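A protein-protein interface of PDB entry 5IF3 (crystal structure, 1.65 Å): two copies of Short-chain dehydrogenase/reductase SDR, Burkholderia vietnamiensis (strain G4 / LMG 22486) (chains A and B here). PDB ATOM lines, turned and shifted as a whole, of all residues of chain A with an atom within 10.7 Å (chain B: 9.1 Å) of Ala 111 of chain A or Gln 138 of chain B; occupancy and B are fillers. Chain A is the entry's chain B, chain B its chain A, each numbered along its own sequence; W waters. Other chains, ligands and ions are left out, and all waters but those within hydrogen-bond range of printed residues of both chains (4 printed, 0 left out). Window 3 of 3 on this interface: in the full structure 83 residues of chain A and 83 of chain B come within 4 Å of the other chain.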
ATOM      1  N   PRO A 106      -6.831  23.789  12.935  1.00  0.00           N
ATOM      2  CA  PRO A 106      -5.618  23.740  13.755  1.00  0.00           C
ATOM      3  C   PRO A 106      -4.679  22.601  13.381  1.00  0.00           C
ATOM      4  O   PRO A 106      -5.083  21.434  13.338  1.00  0.00           O
ATOM      5  CB  PRO A 106      -6.174  23.540  15.177  1.00  0.00           C
ATOM      6  CG  PRO A 106      -7.416  22.736  14.958  1.00  0.00           C
ATOM      7  CD  PRO A 106      -7.979  23.160  13.615  1.00  0.00           C
ATOM      8  N   ILE A 107      -3.430  22.969  13.124  1.00  0.00           N
ATOM      9  CA  ILE A 107      -2.383  22.013  12.794  1.00  0.00           C
ATOM     10  C   ILE A 107      -1.744  21.518  14.086  1.00  0.00           C
ATOM     11  O   ILE A 107      -1.428  22.312  14.981  1.00  0.00           O
ATOM     12  CB  ILE A 107      -1.332  22.652  11.871  1.00  0.00           C
ATOM     13  CG1 ILE A 107      -1.956  23.019  10.526  1.00  0.00           C
ATOM     14  CG2 ILE A 107      -0.152  21.712  11.663  1.00  0.00           C
ATOM     15  CD1 ILE A 107      -1.012  23.767   9.608  1.00  0.00           C
ATOM     16  N   GLY A 108      -1.546  20.212  14.172  1.00  0.00           N
ATOM     17  CA  GLY A 108      -0.904  19.597  15.304  1.00  0.00           C
ATOM     18  C   GLY A 108      -1.631  18.343  15.740  1.00  0.00           C
ATOM     19  O   GLY A 108      -2.695  17.991  15.213  1.00  0.00           O
ATOM     20  N   PRO A 109      -1.059  17.641  16.719  1.00  0.00           N
ATOM     21  CA  PRO A 109      -1.719  16.458  17.282  1.00  0.00           C
ATOM     22  C   PRO A 109      -2.934  16.859  18.103  1.00  0.00           C
ATOM     23  O   PRO A 109      -3.132  18.037  18.405  1.00  0.00           O
ATOM     24  CB  PRO A 109      -0.645  15.855  18.187  1.00  0.00           C
ATOM     25  CG  PRO A 109       0.138  17.074  18.650  1.00  0.00           C
ATOM     26  CD  PRO A 109       0.193  17.970  17.427  1.00  0.00           C
ATOM     27  N   LEU A 110      -3.728  15.850  18.479  1.00  0.00           N
ATOM     28  CA  LEU A 110      -4.922  16.120  19.284  1.00  0.00           C
ATOM     29  C   LEU A 110      -4.601  16.960  20.515  1.00  0.00           C
ATOM     30  O   LEU A 110      -5.403  17.818  20.907  1.00  0.00           O
ATOM     31  CB  LEU A 110      -5.602  14.818  19.714  1.00  0.00           C
ATOM     32  CG  LEU A 110      -6.290  14.034  18.593  1.00  0.00           C
ATOM     33  CD1 LEU A 110      -6.948  12.813  19.202  1.00  0.00           C
ATOM     34  CD2 LEU A 110      -7.306  14.910  17.856  1.00  0.00           C
ATOM     35  N   ALA A 111      -3.441  16.728  21.147  1.00  0.00           N
ATOM     36  CA  ALA A 111      -3.107  17.459  22.372  1.00  0.00           C
ATOM     37  C   ALA A 111      -2.975  18.957  22.144  1.00  0.00           C
ATOM     38  O   ALA A 111      -3.042  19.730  23.115  1.00  0.00           O
ATOM     39  CB  ALA A 111      -1.810  16.921  22.981  1.00  0.00           C
ATOM     40  N   ALA A 112      -2.773  19.384  20.896  1.00  0.00           N
ATOM     41  CA  ALA A 112      -2.496  20.779  20.596  1.00  0.00           C
ATOM     42  C   ALA A 112      -3.671  21.529  19.980  1.00  0.00           C
ATOM     43  O   ALA A 112      -3.607  22.759  19.879  1.00  0.00           O
ATOM     44  CB  ALA A 112      -1.285  20.866  19.651  1.00  0.00           C
ATOM     45  N   GLN A 113      -4.751  20.844  19.599  1.00  0.00           N
ATOM     46  CA  GLN A 113      -5.812  21.451  18.801  1.00  0.00           C
ATOM     47  C   GLN A 113      -6.842  22.151  19.681  1.00  0.00           C
ATOM     48  O   GLN A 113      -7.497  21.501  20.503  1.00  0.00           O
ATOM     49  CB  GLN A 113      -6.523  20.387  17.964  1.00  0.00           C
ATOM     50  CG  GLN A 113      -5.657  19.688  16.945  1.00  0.00           C
ATOM     51  CD  GLN A 113      -6.411  18.531  16.299  1.00  0.00           C
ATOM     52  OE1 GLN A 113      -7.620  18.369  16.498  1.00  0.00           O
ATOM     53  NE2 GLN A 113      -5.692  17.722  15.526  1.00  0.00           N
ATOM     54  N   ASP A 114      -7.044  23.445  19.456  1.00  0.00           N
ATOM     55  CA  ASP A 114      -8.125  24.174  20.141  1.00  0.00           C
ATOM     56  C   ASP A 114      -9.469  23.655  19.640  1.00  0.00           C
ATOM     57  O   ASP A 114      -9.725  23.710  18.430  1.00  0.00           O
ATOM     58  CB  ASP A 114      -7.979  25.676  19.862  1.00  0.00           C
ATOM     59  CG  ASP A 114      -9.033  26.531  20.562  1.00  0.00           C
ATOM     60  OD1 ASP A 114     -10.008  26.000  21.136  1.00  0.00           O
ATOM     61  OD2 ASP A 114      -8.859  27.774  20.551  1.00  0.00           O
ATOM     62  N   PRO A 115     -10.345  23.129  20.504  1.00  0.00           N
ATOM     63  CA  PRO A 115     -11.642  22.643  20.003  1.00  0.00           C
ATOM     64  C   PRO A 115     -12.445  23.702  19.264  1.00  0.00           C
ATOM     65  O   PRO A 115     -13.165  23.361  18.313  1.00  0.00           O
ATOM     66  CB  PRO A 115     -12.357  22.177  21.286  1.00  0.00           C
ATOM     67  CG  PRO A 115     -11.234  21.757  22.182  1.00  0.00           C
ATOM     68  CD  PRO A 115     -10.139  22.780  21.920  1.00  0.00           C
ATOM     69  N   ALA A 116     -12.331  24.976  19.659  1.00  0.00           N
ATOM     70  CA  ALA A 116     -13.036  26.038  18.947  1.00  0.00           C
ATOM     71  C   ALA A 116     -12.555  26.152  17.502  1.00  0.00           C
ATOM     72  O   ALA A 116     -13.357  26.386  16.589  1.00  0.00           O
ATOM     73  CB  ALA A 116     -12.858  27.369  19.679  1.00  0.00           C
ATOM     74  N   LEU A 117     -11.248  25.991  17.272  1.00  0.00           N
ATOM     75  CA  LEU A 117     -10.731  26.026  15.903  1.00  0.00           C
ATOM     76  C   LEU A 117     -11.086  24.761  15.134  1.00  0.00           C
ATOM     77  O   LEU A 117     -11.251  24.804  13.909  1.00  0.00           O
ATOM     78  CB  LEU A 117      -9.220  26.223  15.918  1.00  0.00           C
ATOM     79  CG  LEU A 117      -8.732  27.587  16.410  1.00  0.00           C
ATOM     80  CD1 LEU A 117      -7.223  27.618  16.413  1.00  0.00           C
ATOM     81  CD2 LEU A 117      -9.298  28.690  15.533  1.00  0.00           C
ATOM     82  N   VAL A 118     -11.175  23.622  15.825  1.00  0.00           N
ATOM     83  CA  VAL A 118     -11.682  22.410  15.186  1.00  0.00           C
ATOM     84  C   VAL A 118     -13.077  22.662  14.638  1.00  0.00           C
ATOM     85  O   VAL A 118     -13.372  22.366  13.472  1.00  0.00           O
ATOM     86  CB  VAL A 118     -11.684  21.237  16.182  1.00  0.00           C
ATOM     87  CG1 VAL A 118     -12.343  19.998  15.545  1.00  0.00           C
ATOM     88  CG2 VAL A 118     -10.266  20.901  16.631  1.00  0.00           C
ATOM     89  N   GLY A 162      -0.140  15.674  11.902  1.00  0.00           N
ATOM     90  CA  GLY A 162      -0.429  17.069  12.157  1.00  0.00           C
ATOM     91  C   GLY A 162      -1.647  17.609  11.438  1.00  0.00           C
ATOM     92  O   GLY A 162      -2.180  18.648  11.833  1.00  0.00           O
ATOM     93  N   SER A 164      -4.728  16.121  10.877  1.00  0.00           N
ATOM     94  CA  SER A 164      -5.894  15.253  11.006  1.00  0.00           C
ATOM     95  C   SER A 164      -7.203  15.994  10.753  1.00  0.00           C
ATOM     96  O   SER A 164      -8.146  15.411  10.195  1.00  0.00           O
ATOM     97  CB  SER A 164      -5.909  14.573  12.384  1.00  0.00           C
ATOM     98  OG  SER A 164      -5.900  15.505  13.458  1.00  0.00           O
ATOM     99  N   VAL A 165      -7.294  17.266  11.131  1.00  0.00           N
ATOM    100  CA  VAL A 165      -8.545  17.982  10.917  1.00  0.00           C
ATOM    101  C   VAL A 165      -8.743  18.272   9.432  1.00  0.00           C
ATOM    102  O   VAL A 165      -9.795  17.967   8.856  1.00  0.00           O
ATOM    103  CB  VAL A 165      -8.586  19.260  11.771  1.00  0.00           C
ATOM    104  CG1 VAL A 165      -9.863  20.046  11.476  1.00  0.00           C
ATOM    105  CG2 VAL A 165      -8.488  18.889  13.263  1.00  0.00           C
ATOM    106  N   LEU B  80     -16.848  22.097  26.878  1.00  0.00           N
ATOM    107  CA  LEU B  80     -15.471  21.609  26.919  1.00  0.00           C
ATOM    108  C   LEU B  80     -14.528  22.618  27.562  1.00  0.00           C
ATOM    109  O   LEU B  80     -13.494  22.228  28.116  1.00  0.00           O
ATOM    110  CB  LEU B  80     -14.981  21.275  25.508  1.00  0.00           C
ATOM    111  CG  LEU B  80     -15.670  20.103  24.818  1.00  0.00           C
ATOM    112  CD1 LEU B  80     -15.160  19.986  23.364  1.00  0.00           C
ATOM    113  CD2 LEU B  80     -15.416  18.818  25.567  1.00  0.00           C
ATOM    114  N   ALA B  81     -14.846  23.911  27.470  1.00  0.00           N
ATOM    115  CA  ALA B  81     -14.059  24.917  28.169  1.00  0.00           C
ATOM    116  C   ALA B  81     -14.329  24.902  29.666  1.00  0.00           C
ATOM    117  O   ALA B  81     -13.549  25.483  30.431  1.00  0.00           O
ATOM    118  CB  ALA B  81     -14.349  26.304  27.602  1.00  0.00           C
ATOM    119  N   LEU B  85     -15.507  17.474  31.860  1.00  0.00           N
ATOM    120  CA  LEU B  85     -14.754  16.358  31.307  1.00  0.00           C
ATOM    121  C   LEU B  85     -13.508  16.076  32.137  1.00  0.00           C
ATOM    122  O   LEU B  85     -13.200  14.918  32.437  1.00  0.00           O
ATOM    123  CB  LEU B  85     -14.388  16.655  29.851  1.00  0.00           C
ATOM    124  CG  LEU B  85     -13.612  15.542  29.161  1.00  0.00           C
ATOM    125  CD1 LEU B  85     -14.395  14.263  29.179  1.00  0.00           C
ATOM    126  CD2 LEU B  85     -13.249  15.955  27.722  1.00  0.00           C
ATOM    127  N   ARG B  86     -12.773  17.124  32.514  1.00  0.00           N
ATOM    128  CA  ARG B  86     -11.587  16.927  33.338  1.00  0.00           C
ATOM    129  C   ARG B  86     -11.951  16.260  34.664  1.00  0.00           C
ATOM    130  O   ARG B  86     -11.251  15.353  35.131  1.00  0.00           O
ATOM    131  CB  ARG B  86     -10.888  18.269  33.570  1.00  0.00           C
ATOM    132  CG  ARG B  86      -9.601  18.188  34.354  1.00  0.00           C
ATOM    133  CD  ARG B  86      -8.825  19.498  34.278  1.00  0.00           C
ATOM    134  NE  ARG B  86      -9.597  20.673  34.690  1.00  0.00           N
ATOM    135  CZ  ARG B  86     -10.226  21.495  33.850  1.00  0.00           C
ATOM    136  NH1 ARG B  86     -10.192  21.269  32.541  1.00  0.00           N
ATOM    137  NH2 ARG B  86     -10.898  22.537  34.318  1.00  0.00           N
ATOM    138  N   VAL B  89     -12.517  12.442  34.104  1.00  0.00           N
ATOM    139  CA  VAL B  89     -11.360  11.604  33.798  1.00  0.00           C
ATOM    140  C   VAL B  89     -10.250  11.687  34.840  1.00  0.00           C
ATOM    141  O   VAL B  89      -9.331  10.855  34.805  1.00  0.00           O
ATOM    142  CB  VAL B  89     -10.776  11.947  32.413  1.00  0.00           C
ATOM    143  CG1 VAL B  89     -11.856  11.808  31.340  1.00  0.00           C
ATOM    144  CG2 VAL B  89     -10.195  13.345  32.412  1.00  0.00           C
ATOM    145  N   LEU B 130     -14.658  15.251  16.566  1.00  0.00           N
ATOM    146  CA  LEU B 130     -13.300  15.766  16.443  1.00  0.00           C
ATOM    147  C   LEU B 130     -12.961  16.671  17.624  1.00  0.00           C
ATOM    148  O   LEU B 130     -11.828  16.652  18.119  1.00  0.00           O
ATOM    149  CB  LEU B 130     -13.121  16.495  15.107  1.00  0.00           C
ATOM    150  CG  LEU B 130     -12.633  15.630  13.938  1.00  0.00           C
ATOM    151  CD1 LEU B 130     -13.556  14.419  13.754  1.00  0.00           C
ATOM    152  CD2 LEU B 130     -12.580  16.476  12.676  1.00  0.00           C
ATOM    153  N   MET B 131     -13.940  17.446  18.100  1.00  0.00           N
ATOM    154  CA  MET B 131     -13.709  18.301  19.266  1.00  0.00           C
ATOM    155  C   MET B 131     -13.529  17.472  20.530  1.00  0.00           C
ATOM    156  O   MET B 131     -12.628  17.739  21.341  1.00  0.00           O
ATOM    157  CB  MET B 131     -14.875  19.282  19.442  1.00  0.00           C
ATOM    158  CG  MET B 131     -14.999  20.327  18.320  1.00  0.00           C
ATOM    159  SD  MET B 131     -16.626  21.117  18.414  1.00  0.00           S
ATOM    160  CE  MET B 131     -16.336  22.264  19.748  1.00  0.00           C
ATOM    161  N   LEU B 132     -14.389  16.463  20.728  1.00  0.00           N
ATOM    162  CA  LEU B 132     -14.284  15.638  21.926  1.00  0.00           C
ATOM    163  C   LEU B 132     -12.998  14.831  21.954  1.00  0.00           C
ATOM    164  O   LEU B 132     -12.441  14.598  23.039  1.00  0.00           O
ATOM    165  CB  LEU B 132     -15.490  14.697  22.027  1.00  0.00           C
ATOM    166  CG  LEU B 132     -16.836  15.357  22.315  1.00  0.00           C
ATOM    167  CD1 LEU B 132     -17.971  14.344  22.041  1.00  0.00           C
ATOM    168  CD2 LEU B 132     -16.902  15.851  23.738  1.00  0.00           C
ATOM    169  N   SER B 133     -12.504  14.410  20.781  1.00  0.00           N
ATOM    170  CA  SER B 133     -11.250  13.674  20.741  1.00  0.00           C
ATOM    171  C   SER B 133     -10.111  14.551  21.234  1.00  0.00           C
ATOM    172  O   SER B 133      -9.311  14.131  22.073  1.00  0.00           O
ATOM    173  CB  SER B 133     -10.953  13.195  19.322  1.00  0.00           C
ATOM    174  OG  SER B 133     -11.984  12.323  18.869  1.00  0.00           O
ATOM    175  N   ALA B 134     -10.014  15.765  20.694  1.00  0.00           N
ATOM    176  CA  ALA B 134      -8.985  16.694  21.154  1.00  0.00           C
ATOM    177  C   ALA B 134      -9.146  17.001  22.644  1.00  0.00           C
ATOM    178  O   ALA B 134      -8.161  16.997  23.395  1.00  0.00           O
ATOM    179  CB  ALA B 134      -9.032  17.991  20.336  1.00  0.00           C
ATOM    180  N   ALA B 135     -10.380  17.254  23.097  1.00  0.00           N
ATOM    181  CA  ALA B 135     -10.565  17.666  24.488  1.00  0.00           C
ATOM    182  C   ALA B 135     -10.230  16.538  25.452  1.00  0.00           C
ATOM    183  O   ALA B 135      -9.710  16.791  26.547  1.00  0.00           O
ATOM    184  CB  ALA B 135     -12.000  18.140  24.710  1.00  0.00           C
ATOM    185  N   LEU B 136     -10.552  15.288  25.090  1.00  0.00           N
ATOM    186  CA  LEU B 136     -10.224  14.175  25.981  1.00  0.00           C
ATOM    187  C   LEU B 136      -8.720  14.076  26.194  1.00  0.00           C
ATOM    188  O   LEU B 136      -8.245  13.967  27.328  1.00  0.00           O
ATOM    189  CB  LEU B 136     -10.765  12.854  25.423  1.00  0.00           C
ATOM    190  CG  LEU B 136     -10.249  11.636  26.191  1.00  0.00           C
ATOM    191  CD1 LEU B 136     -10.689  11.677  27.653  1.00  0.00           C
ATOM    192  CD2 LEU B 136     -10.752  10.328  25.501  1.00  0.00           C
ATOM    193  N   VAL B 137      -7.952  14.102  25.104  1.00  0.00           N
ATOM    194  CA  VAL B 137      -6.500  14.030  25.233  1.00  0.00           C
ATOM    195  C   VAL B 137      -5.981  15.170  26.094  1.00  0.00           C
ATOM    196  O   VAL B 137      -5.067  14.989  26.914  1.00  0.00           O
ATOM    197  CB  VAL B 137      -5.862  14.021  23.834  1.00  0.00           C
ATOM    198  CG1 VAL B 137      -4.361  14.221  23.924  1.00  0.00           C
ATOM    199  CG2 VAL B 137      -6.207  12.702  23.140  1.00  0.00           C
ATOM    200  N   GLN B 138      -6.587  16.352  25.964  1.00  0.00           N
ATOM    201  CA  GLN B 138      -6.125  17.514  26.712  1.00  0.00           C
ATOM    202  C   GLN B 138      -6.581  17.517  28.164  1.00  0.00           C
ATOM    203  O   GLN B 138      -5.972  18.216  28.983  1.00  0.00           O
ATOM    204  CB  GLN B 138      -6.611  18.792  26.032  1.00  0.00           C
ATOM    205  CG  GLN B 138      -5.972  18.964  24.649  1.00  0.00           C
ATOM    206  CD  GLN B 138      -6.590  20.077  23.849  1.00  0.00           C
ATOM    207  OE1 GLN B 138      -7.119  21.039  24.402  1.00  0.00           O
ATOM    208  NE2 GLN B 138      -6.515  19.959  22.521  1.00  0.00           N
ATOM    209  N   ALA B 139      -7.639  16.766  28.493  1.00  0.00           N
ATOM    210  CA  ALA B 139      -8.137  16.701  29.865  1.00  0.00           C
ATOM    211  C   ALA B 139      -7.468  15.602  30.676  1.00  0.00           C
ATOM    212  O   ALA B 139      -7.464  15.661  31.910  1.00  0.00           O
ATOM    213  CB  ALA B 139      -9.655  16.454  29.860  1.00  0.00           C
ATOM    214  N   ALA B 140      -6.948  14.575  30.000  1.00  0.00           N
ATOM    215  CA  ALA B 140      -6.411  13.386  30.653  1.00  0.00           C
ATOM    216  C   ALA B 140      -4.932  13.597  30.946  1.00  0.00           C
ATOM    217  O   ALA B 140      -4.095  13.554  30.040  1.00  0.00           O
ATOM    218  CB  ALA B 140      -6.611  12.158  29.767  1.00  0.00           C
ATOM    219  N   ALA B 141      -4.604  13.793  32.203  1.00  0.00           N
ATOM    220  CA  ALA B 141      -3.203  13.983  32.545  1.00  0.00           C
ATOM    221  C   ALA B 141      -2.498  12.636  32.625  1.00  0.00           C
ATOM    222  O   ALA B 141      -3.124  11.591  32.801  1.00  0.00           O
ATOM    223  CB  ALA B 141      -3.077  14.734  33.865  1.00  0.00           C
ATOM    224  N   ALA B 142      -1.179  12.664  32.463  1.00  0.00           N
ATOM    225  CA  ALA B 142      -0.392  11.463  32.659  1.00  0.00           C
ATOM    226  C   ALA B 142      -0.690  10.903  34.050  1.00  0.00           C
ATOM    227  O   ALA B 142      -0.846  11.677  35.005  1.00  0.00           O
ATOM    228  CB  ALA B 142       1.105  11.773  32.514  1.00  0.00           C
ATOM    229  N   CYS B 146      -5.717   6.995  26.768  1.00  0.00           N
ATOM    230  CA  CYS B 146      -6.960   7.315  26.079  1.00  0.00           C
ATOM    231  C   CYS B 146      -7.125   6.394  24.887  1.00  0.00           C
ATOM    232  O   CYS B 146      -6.157   6.124  24.168  1.00  0.00           O
ATOM    233  CB  CYS B 146      -6.984   8.756  25.571  1.00  0.00           C
ATOM    234  SG  CYS B 146      -6.996   9.973  26.950  1.00  0.00           S
ATOM    235  N   VAL B 180      -4.564  10.893  12.805  1.00  0.00           N
ATOM    236  CA  VAL B 180      -4.215  10.918  14.229  1.00  0.00           C
ATOM    237  C   VAL B 180      -3.224   9.807  14.548  1.00  0.00           C
ATOM    238  O   VAL B 180      -2.305   9.976  15.364  1.00  0.00           O
ATOM    239  CB  VAL B 180      -5.489  10.814  15.089  1.00  0.00           C
ATOM    240  CG1 VAL B 180      -5.144  10.504  16.561  1.00  0.00           C
ATOM    241  CG2 VAL B 180      -6.303  12.098  14.987  1.00  0.00           C
ATOM    242  N   ASP B 183       0.449  10.755  14.382  1.00  0.00           N
ATOM    243  CA  ASP B 183       0.956  11.765  15.296  1.00  0.00           C
ATOM    244  C   ASP B 183       1.734  11.123  16.436  1.00  0.00           C
ATOM    245  O   ASP B 183       1.539   9.957  16.774  1.00  0.00           O
ATOM    246  CB  ASP B 183      -0.200  12.581  15.876  1.00  0.00           C
ATOM    247  CG  ASP B 183      -0.803  13.554  14.872  1.00  0.00           C
ATOM    248  OD1 ASP B 183      -0.062  14.070  14.013  1.00  0.00           O
ATOM    249  OD2 ASP B 183      -2.021  13.822  14.975  1.00  0.00           O
ATOM    250  N   ALA B 184       2.629  11.920  17.043  1.00  0.00           N
ATOM    251  CA  ALA B 184       3.307  11.559  18.288  1.00  0.00           C
ATOM    252  C   ALA B 184       2.407  11.954  19.455  1.00  0.00           C
ATOM    253  O   ALA B 184       2.404  13.112  19.902  1.00  0.00           O
ATOM    254  CB  ALA B 184       4.665  12.244  18.398  1.00  0.00           C
ATOM    255  N   ASN B 185       1.669  10.975  19.949  1.00  0.00           N
ATOM    256  CA  ASN B 185       0.726  11.113  21.052  1.00  0.00           C
ATOM    257  C   ASN B 185       1.302  10.447  22.295  1.00  0.00           C
ATOM    258  O   ASN B 185       2.085   9.499  22.201  1.00  0.00           O
ATOM    259  CB  ASN B 185      -0.617  10.461  20.688  1.00  0.00           C
ATOM    260  CG  ASN B 185      -1.181  10.956  19.345  1.00  0.00           C
ATOM    261  OD1 ASN B 185      -1.396  12.157  19.176  1.00  0.00           O
ATOM    262  ND2 ASN B 185      -1.402  10.036  18.386  1.00  0.00           N
ATOM    263  N   ARG B 186       0.906  10.936  23.473  1.00  0.00           N
ATOM    264  CA  ARG B 186       1.457  10.369  24.705  1.00  0.00           C
ATOM    265  C   ARG B 186       1.027   8.918  24.898  1.00  0.00           C
ATOM    266  O   ARG B 186       1.861   8.018  25.077  1.00  0.00           O
ATOM    267  CB  ARG B 186       1.030  11.192  25.921  1.00  0.00           C
ATOM    268  CG  ARG B 186       1.677  10.663  27.199  1.00  0.00           C
ATOM    269  CD  ARG B 186       1.369  11.479  28.472  1.00  0.00           C
ATOM    270  NE  ARG B 186      -0.046  11.745  28.680  1.00  0.00           N
ATOM    271  CZ  ARG B 186      -0.910  10.882  29.211  1.00  0.00           C
ATOM    272  NH1 ARG B 186      -0.511   9.666  29.584  1.00  0.00           N
ATOM    273  NH2 ARG B 186      -2.183  11.231  29.367  1.00  0.00           N
ATOM    274  N   ALA B 187      -0.275   8.684  24.917  1.00  0.00           N
ATOM    275  CA  ALA B 187      -0.833   7.377  25.256  1.00  0.00           C
ATOM    276  C   ALA B 187      -2.219   7.331  24.654  1.00  0.00           C
ATOM    277  O   ALA B 187      -3.227   7.456  25.359  1.00  0.00           O
ATOM    278  CB  ALA B 187      -0.888   7.150  26.767  1.00  0.00           C
ATOM    279  N   LEU B 188      -2.262   7.211  23.340  1.00  0.00           N
ATOM    280  CA  LEU B 188      -3.499   7.324  22.579  1.00  0.00           C
ATOM    281  C   LEU B 188      -3.556   6.213  21.552  1.00  0.00           C
ATOM    282  O   LEU B 188      -2.591   5.992  20.809  1.00  0.00           O
ATOM    283  CB  LEU B 188      -3.583   8.682  21.869  1.00  0.00           C
ATOM    284  CG  LEU B 188      -4.805   8.864  20.969  1.00  0.00           C
ATOM    285  CD1 LEU B 188      -6.099   8.894  21.788  1.00  0.00           C
ATOM    286  CD2 LEU B 188      -4.676  10.111  20.132  1.00  0.00           C
HETATM  287  O   HOH W   1      -3.084  13.318  17.430  1.00  0.00           O
HETATM  288  O   HOH W   2      -9.687  16.586  16.073  1.00  0.00           O
HETATM  289  O   HOH W   3      -3.132  15.760  13.538  1.00  0.00           O
HETATM  290  O   HOH W   4      -1.792  14.205  21.008  1.00  0.00           O
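NE2 of Gln 138 of chain B is in hydrogen-bond range of O of Gln 113 of chain A. OD1 of Asp 183 of chain B is in hydrogen-bond range of N of Gly 162 of chain A. NE2 of Gln 138 of chain B sits at hydrogen-bond distance from O of Leu 110 of chain A.
The side-chain hydroxyl of Ser 164 of chain A is in hydrogen-bond range of the side-chain amide nitrogen of Gln 113 of chain A, at 3.0 Å. The backbone carbonyl oxygen of Asp 183 of chain B is in hydrogen-bond range of the side-chain amide nitrogen of Asn 185 of chain B, at 3.4 Å. The backbone carbonyl oxygen (O) of Val 180 of chain B lies within hydrogen-bond range of the side-chain amide nitrogen (ND2) of Asn 185 of chain B. N of Gly 108 of chain A sits at hydrogen-bond distance from O of Gly 162 of chain A (2.9 Å). The backbone carbonyl oxygen of Gly 108 of chain A lies within hydrogen-bond range of the side-chain amide nitrogen of Gln 113 of chain A (3.0 Å). O of Ala 134 of chain B sits close to NE2 of Gln 138 of chain B.
Asp 183 of chain B touches Pro 109 of chain A (OD2 to CA, 3.5 Å). Ser 133 of chain B touches Leu 110 of chain A. CB of Ala 134 of chain B touches O of Leu 110 of chain A, 3.7 Å away. Leu 110 of chain A touches Val 180 of chain B (CD1 to CG1, 3.9 Å). CD1 of Leu 110 of chain A touches CD2 of Leu 188 of chain B, 3.7 Å away. CA of Ala 111 of chain A touches CG1 of Val 137 of chain B, 3.8 Å away. Ala 111 of chain A touches Gln 138 of chain B (O to CG, 3.4 Å). O of Pro 115 of chain A touches CG of Met 131 of chain B, at 3.5 Å. Val 118 of chain A touches Leu 130 of chain B. CB of Ser 164 of chain A touches CG2 of Val 180 of chain B, 3.6 Å away.
Of chain B, only Val 137 (3.8 Å) and Gln 138 (3.4 Å) come within 4 Å of Ala 111 of chain A. Gln 138 of chain B touches three residues of chain A. No residue of chain A comes within 4 Å of Ala 135 of chain B. No residue of chain A comes within 4 Å of Ala 140 of chain B. Of the printed residues of chain A, Leu 188 of chain B touches Leu 110. Of the printed residues of chain A, Ser 133 of chain B touches Leu 110. Of the printed residues of chain A, Val 180 of chain B touches Leu 110 (3.9 Å) and Ser 164 (3.6 Å). Printed residues of chain A within 4 Å of Met 131 of chain B: Pro 115 and Val 118. Of the printed residues of chain A, Leu 130 of chain B touches Val 118. The nearest residue of chain B that does not touch Ala 111 of chain A is Ala 134 of chain B (5.2 Å). The nearest residue of chain A that does not touch Gln 138 of chain B is Ala 112 of chain A (4.1 Å). The nearest printed residue of chain A that does not touch Met 131 of chain B is Ala 116 of chain A (4.8 Å).
Of the 26 printed residues of chain B, 10 touch a printed residue of chain A. Hydrophobic or aromatic side chains of chain B that line the printed part of chain A: Leu 130, Met 131, Ala 134, Val 137, Val 180 and Leu 188. Among the printed residues, 16 pairs touch across the chains.
No position is printed for both chains. Of the 16 pairs that touch across the chains among the printed residues, none has its exchanged pair printed and touching as well.
Water W3 lies within hydrogen-bond range of OD2 of Asp 183 of chain B (2.7 Å), OG of Ser 164 of chain A (2.8 Å), O of Gly 108 of chain A (2.8 Å) and N of Gly 162 of chain A (3.4 Å). Water W1 lies within hydrogen-bond range of the side-chain amide oxygen of Asn 185 of chain B (2.7 Å), the side-chain carboxylate of Asp 183 of chain B (2.7 Å) and the backbone NH of Leu 110 of chain A (2.8 Å). Water W2 bridges OE1 of Gln 113 of chain A (2.8 Å) and O of Leu 130 of chain B (3.0 Å). Water W4 lies within hydrogen-bond range of the side-chain amide oxygen of Asn 185 of chain B and the backbone NH of Ala 111 of chain A.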
